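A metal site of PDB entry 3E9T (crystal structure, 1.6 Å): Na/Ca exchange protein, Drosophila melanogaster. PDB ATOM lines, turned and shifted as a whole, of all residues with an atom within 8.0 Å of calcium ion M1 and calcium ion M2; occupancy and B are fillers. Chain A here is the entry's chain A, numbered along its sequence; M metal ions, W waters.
Water W1 bridges the side-chain carboxylate (OD2) of Asp 111 and the backbone carbonyl oxygen (O) of Asp 78.
Within 4 Å of calcium ion M1: Glu 16, Asp 77, Val 79, Glu 81 and Asp 111.
OD2 of Asp 111 lies close to N of Glu 81 (3.4 Å). The side-chain carboxylate of Asp 112 sits close to the side-chain amide nitrogen of Asn 17, at 3.2 Å. The backbone carbonyl oxygen (O) of Leu 110 sits at hydrogen-bond distance from the backbone NH (N) of Glu 16, at 2.8 Å.
Calcium ion M1 is bound by the backbone carbonyl oxygen (O) of Val 79 (2.2 Å), the side-chain carboxylate (OD2) of Asp 77 (2.4 Å), the side-chain carboxylate (OE2) of Glu 16 (2.4 Å), the side-chain carboxylate (OD1) of Asp 111 (2.4 Å), water W1 (2.5 Å) and the side-chain carboxylate (OE1) of Glu 16 (2.7 Å). Calcium ion M1 has six donor atoms within binding distance. Slightly farther from calcium ion M1 lies OE1 of Glu 81 (3.0 Å).
Calcium ion M2 is bound by the side-chain carboxylate (OD1) of Asp 112, the side-chain carboxylate (OD2) of Asp 76, the side-chain carboxylate (OE2) of Glu 16, the backbone carbonyl oxygen (O) of Asp 77 and water W1.
Within 4 Å of calcium ion M2: Glu 16, Asp 76, Asp 77 and Asp 112.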
ATOM      1  N   MET A  15      -7.989 -13.208 -21.775  1.00  0.00           N
ATOM      2  CA  MET A  15      -8.559 -12.641 -22.991  1.00  0.00           C
ATOM      3  C   MET A  15      -8.553 -13.688 -24.089  1.00  0.00           C
ATOM      4  O   MET A  15      -7.650 -14.521 -24.156  1.00  0.00           O
ATOM      5  CB  MET A  15      -7.767 -11.401 -23.448  1.00  0.00           C
ATOM      6  CG  MET A  15      -7.599 -10.366 -22.341  1.00  0.00           C
ATOM      7  SD  MET A  15      -9.187  -9.789 -21.682  1.00  0.00           S
ATOM      8  CE  MET A  15      -9.964  -9.081 -23.110  1.00  0.00           C
ATOM      9  N   GLU A  16      -9.564 -13.628 -24.943  1.00  0.00           N
ATOM     10  CA  GLU A  16      -9.724 -14.571 -26.047  1.00  0.00           C
ATOM     11  C   GLU A  16      -8.498 -14.681 -26.984  1.00  0.00           C
ATOM     12  O   GLU A  16      -8.275 -15.726 -27.600  1.00  0.00           O
ATOM     13  CB  GLU A  16     -10.956 -14.191 -26.854  1.00  0.00           C
ATOM     14  CG  GLU A  16     -11.270 -15.199 -27.919  1.00  0.00           C
ATOM     15  CD  GLU A  16     -12.423 -14.784 -28.766  1.00  0.00           C
ATOM     16  OE1 GLU A  16     -13.370 -15.585 -28.893  1.00  0.00           O
ATOM     17  OE2 GLU A  16     -12.414 -13.645 -29.283  1.00  0.00           O
ATOM     18  N   ASN A  17      -7.740 -13.606 -27.094  1.00  0.00           N
ATOM     19  CA  ASN A  17      -6.598 -13.543 -28.023  1.00  0.00           C
ATOM     20  C   ASN A  17      -5.266 -13.738 -27.313  1.00  0.00           C
ATOM     21  O   ASN A  17      -4.227 -13.281 -27.791  1.00  0.00           O
ATOM     22  CB  ASN A  17      -6.613 -12.211 -28.797  1.00  0.00           C
ATOM     23  CG  ASN A  17      -6.403 -10.995 -27.893  1.00  0.00           C
ATOM     24  OD1 ASN A  17      -6.705 -11.011 -26.697  1.00  0.00           O
ATOM     25  ND2 ASN A  17      -5.859  -9.930 -28.473  1.00  0.00           N
ATOM     26  N   CYS A  18      -5.293 -14.415 -26.155  1.00  0.00           N
ATOM     27  CA  CYS A  18      -4.084 -14.573 -25.358  1.00  0.00           C
ATOM     28  C   CYS A  18      -3.141 -15.631 -25.936  1.00  0.00           C
ATOM     29  O   CYS A  18      -1.968 -15.647 -25.593  1.00  0.00           O
ATOM     30  CB  CYS A  18      -4.413 -14.924 -23.903  1.00  0.00           C
ATOM     31  SG  CYS A  18      -5.097 -16.594 -23.642  1.00  0.00           S
ATOM     32  N   ASP A  51     -13.641 -22.726 -28.164  1.00  0.00           N
ATOM     33  CA  ASP A  51     -13.172 -21.643 -27.294  1.00  0.00           C
ATOM     34  C   ASP A  51     -11.787 -21.889 -26.703  1.00  0.00           C
ATOM     35  O   ASP A  51     -11.060 -20.938 -26.374  1.00  0.00           O
ATOM     36  CB  ASP A  51     -14.178 -21.417 -26.152  1.00  0.00           C
ATOM     37  CG  ASP A  51     -15.537 -21.049 -26.658  1.00  0.00           C
ATOM     38  OD1 ASP A  51     -16.523 -21.808 -26.444  1.00  0.00           O
ATOM     39  OD2 ASP A  51     -15.632 -19.986 -27.322  1.00  0.00           O
ATOM     40  N   ILE A  75      -8.719 -20.437 -28.103  1.00  0.00           N
ATOM     41  CA  ILE A  75      -9.029 -20.282 -29.507  1.00  0.00           C
ATOM     42  C   ILE A  75      -9.650 -18.905 -29.726  1.00  0.00           C
ATOM     43  O   ILE A  75     -10.664 -18.561 -29.120  1.00  0.00           O
ATOM     44  CB  ILE A  75      -9.968 -21.414 -30.023  1.00  0.00           C
ATOM     45  CG1 ILE A  75      -9.294 -22.793 -29.869  1.00  0.00           C
ATOM     46  CG2 ILE A  75     -10.369 -21.173 -31.488  1.00  0.00           C
ATOM     47  CD1 ILE A  75     -10.180 -23.961 -30.140  1.00  0.00           C
ATOM     48  N   ASP A  76      -9.014 -18.135 -30.602  1.00  0.00           N
ATOM     49  CA  ASP A  76      -9.463 -16.786 -30.947  1.00  0.00           C
ATOM     50  C   ASP A  76     -10.363 -16.848 -32.181  1.00  0.00           C
ATOM     51  O   ASP A  76     -10.142 -17.661 -33.077  1.00  0.00           O
ATOM     52  CB  ASP A  76      -8.241 -15.904 -31.235  1.00  0.00           C
ATOM     53  CG  ASP A  76      -8.557 -14.401 -31.214  1.00  0.00           C
ATOM     54  OD1 ASP A  76      -7.691 -13.621 -31.657  1.00  0.00           O
ATOM     55  OD2 ASP A  76      -9.656 -14.001 -30.756  1.00  0.00           O
ATOM     56  N   ASP A  77     -11.384 -16.001 -32.205  1.00  0.00           N
ATOM     57  CA  ASP A  77     -12.167 -15.797 -33.422  1.00  0.00           C
ATOM     58  C   ASP A  77     -12.526 -14.320 -33.567  1.00  0.00           C
ATOM     59  O   ASP A  77     -12.097 -13.483 -32.762  1.00  0.00           O
ATOM     60  CB  ASP A  77     -13.400 -16.694 -33.453  1.00  0.00           C
ATOM     61  CG  ASP A  77     -14.318 -16.487 -32.260  1.00  0.00           C
ATOM     62  OD1 ASP A  77     -14.824 -17.493 -31.746  1.00  0.00           O
ATOM     63  OD2 ASP A  77     -14.532 -15.325 -31.837  1.00  0.00           O
ATOM     64  N   ASP A  78     -13.314 -13.995 -34.600  1.00  0.00           N
ATOM     65  CA  ASP A  78     -13.779 -12.630 -34.796  1.00  0.00           C
ATOM     66  C   ASP A  78     -15.165 -12.357 -34.211  1.00  0.00           C
ATOM     67  O   ASP A  78     -15.559 -11.205 -34.056  1.00  0.00           O
ATOM     68  CB  ASP A  78     -13.729 -12.246 -36.274  1.00  0.00           C
ATOM     69  CG  ASP A  78     -12.468 -11.495 -36.644  1.00  0.00           C
ATOM     70  OD1 ASP A  78     -11.412 -11.772 -36.026  1.00  0.00           O
ATOM     71  OD2 ASP A  78     -12.518 -10.633 -37.560  1.00  0.00           O
ATOM     72  N   VAL A  79     -15.897 -13.428 -33.895  1.00  0.00           N
ATOM     73  CA  VAL A  79     -17.282 -13.289 -33.425  1.00  0.00           C
ATOM     74  C   VAL A  79     -17.347 -12.770 -31.984  1.00  0.00           C
ATOM     75  O   VAL A  79     -16.589 -13.198 -31.126  1.00  0.00           O
ATOM     76  CB  VAL A  79     -18.049 -14.620 -33.555  1.00  0.00           C
ATOM     77  CG1 VAL A  79     -19.535 -14.431 -33.208  1.00  0.00           C
ATOM     78  CG2 VAL A  79     -17.906 -15.190 -34.969  1.00  0.00           C
ATOM     79  N   PHE A  80     -18.266 -11.824 -31.761  1.00  0.00           N
ATOM     80  CA  PHE A  80     -18.564 -11.297 -30.437  1.00  0.00           C
ATOM     81  C   PHE A  80     -19.170 -12.371 -29.543  1.00  0.00           C
ATOM     82  O   PHE A  80     -20.068 -13.103 -29.960  1.00  0.00           O
ATOM     83  CB  PHE A  80     -19.530 -10.106 -30.602  1.00  0.00           C
ATOM     84  CG  PHE A  80     -20.072  -9.558 -29.299  1.00  0.00           C
ATOM     85  CD1 PHE A  80     -21.411  -9.760 -28.957  1.00  0.00           C
ATOM     86  CD2 PHE A  80     -19.257  -8.826 -28.439  1.00  0.00           C
ATOM     87  CE1 PHE A  80     -21.941  -9.246 -27.771  1.00  0.00           C
ATOM     88  CE2 PHE A  80     -19.768  -8.314 -27.242  1.00  0.00           C
ATOM     89  CZ  PHE A  80     -21.112  -8.517 -26.908  1.00  0.00           C
ATOM     90  N   GLU A  81     -18.638 -12.512 -28.336  1.00  0.00           N
ATOM     91  CA  GLU A  81     -19.197 -13.456 -27.374  1.00  0.00           C
ATOM     92  C   GLU A  81     -19.243 -12.815 -26.007  1.00  0.00           C
ATOM     93  O   GLU A  81     -18.409 -11.972 -25.676  1.00  0.00           O
ATOM     94  CB  GLU A  81     -18.356 -14.741 -27.287  1.00  0.00           C
ATOM     95  CG  GLU A  81     -18.409 -15.605 -28.537  1.00  0.00           C
ATOM     96  CD  GLU A  81     -17.151 -16.441 -28.683  1.00  0.00           C
ATOM     97  OE1 GLU A  81     -16.268 -16.037 -29.477  1.00  0.00           O
ATOM     98  OE2 GLU A  81     -17.031 -17.483 -28.003  1.00  0.00           O
ATOM     99  N   GLU A  82     -20.226 -13.213 -25.227  1.00  0.00           N
ATOM    100  CA  GLU A  82     -20.283 -12.823 -23.833  1.00  0.00           C
ATOM    101  C   GLU A  82     -19.188 -13.564 -23.060  1.00  0.00           C
ATOM    102  O   GLU A  82     -18.577 -14.484 -23.600  1.00  0.00           O
ATOM    103  CB  GLU A  82     -21.679 -13.137 -23.274  1.00  0.00           C
ATOM    104  CG  GLU A  82     -22.762 -12.420 -24.090  1.00  0.00           C
ATOM    105  CD  GLU A  82     -24.190 -12.751 -23.669  1.00  0.00           C
ATOM    106  OE1 GLU A  82     -24.385 -13.564 -22.740  1.00  0.00           O
ATOM    107  OE2 GLU A  82     -25.136 -12.188 -24.282  1.00  0.00           O
ATOM    108  N   ILE A 109     -13.110 -16.720 -20.006  1.00  0.00           N
ATOM    109  CA  ILE A 109     -12.590 -16.093 -21.211  1.00  0.00           C
ATOM    110  C   ILE A 109     -13.357 -14.803 -21.507  1.00  0.00           C
ATOM    111  O   ILE A 109     -14.595 -14.814 -21.605  1.00  0.00           O
ATOM    112  CB  ILE A 109     -12.714 -17.018 -22.448  1.00  0.00           C
ATOM    113  CG1 ILE A 109     -12.023 -18.359 -22.199  1.00  0.00           C
ATOM    114  CG2 ILE A 109     -12.150 -16.323 -23.699  1.00  0.00           C
ATOM    115  CD1 ILE A 109     -12.403 -19.441 -23.250  1.00  0.00           C
ATOM    116  N   LEU A 110     -12.627 -13.699 -21.626  1.00  0.00           N
ATOM    117  CA  LEU A 110     -13.236 -12.432 -22.051  1.00  0.00           C
ATOM    118  C   LEU A 110     -13.005 -12.199 -23.537  1.00  0.00           C
ATOM    119  O   LEU A 110     -11.884 -12.324 -24.011  1.00  0.00           O
ATOM    120  CB  LEU A 110     -12.667 -11.254 -21.249  1.00  0.00           C
ATOM    121  CG  LEU A 110     -12.561 -11.458 -19.732  1.00  0.00           C
ATOM    122  CD1 LEU A 110     -11.938 -10.246 -19.091  1.00  0.00           C
ATOM    123  CD2 LEU A 110     -13.925 -11.745 -19.089  1.00  0.00           C
ATOM    124  N   ASP A 111     -14.071 -11.846 -24.249  1.00  0.00           N
ATOM    125  CA  ASP A 111     -13.979 -11.548 -25.680  1.00  0.00           C
ATOM    126  C   ASP A 111     -13.203 -10.243 -25.933  1.00  0.00           C
ATOM    127  O   ASP A 111     -13.205  -9.328 -25.094  1.00  0.00           O
ATOM    128  CB  ASP A 111     -15.387 -11.436 -26.254  1.00  0.00           C
ATOM    129  CG  ASP A 111     -15.476 -11.891 -27.703  1.00  0.00           C
ATOM    130  OD1 ASP A 111     -15.433 -13.118 -27.947  1.00  0.00           O
ATOM    131  OD2 ASP A 111     -15.595 -11.016 -28.594  1.00  0.00           O
ATOM    132  N   ASP A 112     -12.521 -10.178 -27.072  1.00  0.00           N
ATOM    133  CA  ASP A 112     -11.818  -8.975 -27.505  1.00  0.00           C
ATOM    134  C   ASP A 112     -12.390  -8.541 -28.861  1.00  0.00           C
ATOM    135  O   ASP A 112     -12.756  -7.391 -29.043  1.00  0.00           O
ATOM    136  CB  ASP A 112     -10.320  -9.247 -27.642  1.00  0.00           C
ATOM    137  CG  ASP A 112     -10.006 -10.219 -28.760  1.00  0.00           C
ATOM    138  OD1 ASP A 112     -10.807 -11.153 -29.010  1.00  0.00           O
ATOM    139  OD2 ASP A 112      -8.956 -10.052 -29.409  1.00  0.00           O
HETATM  140 CA    CA M   1     -14.643 -13.637 -30.204  1.00  0.00          CA
HETATM  141 CA    CA M   2     -11.228 -12.305 -30.856  1.00  0.00          CA
HETATM  142  O   HOH W   1     -13.785 -11.546 -31.155  1.00  0.00           O
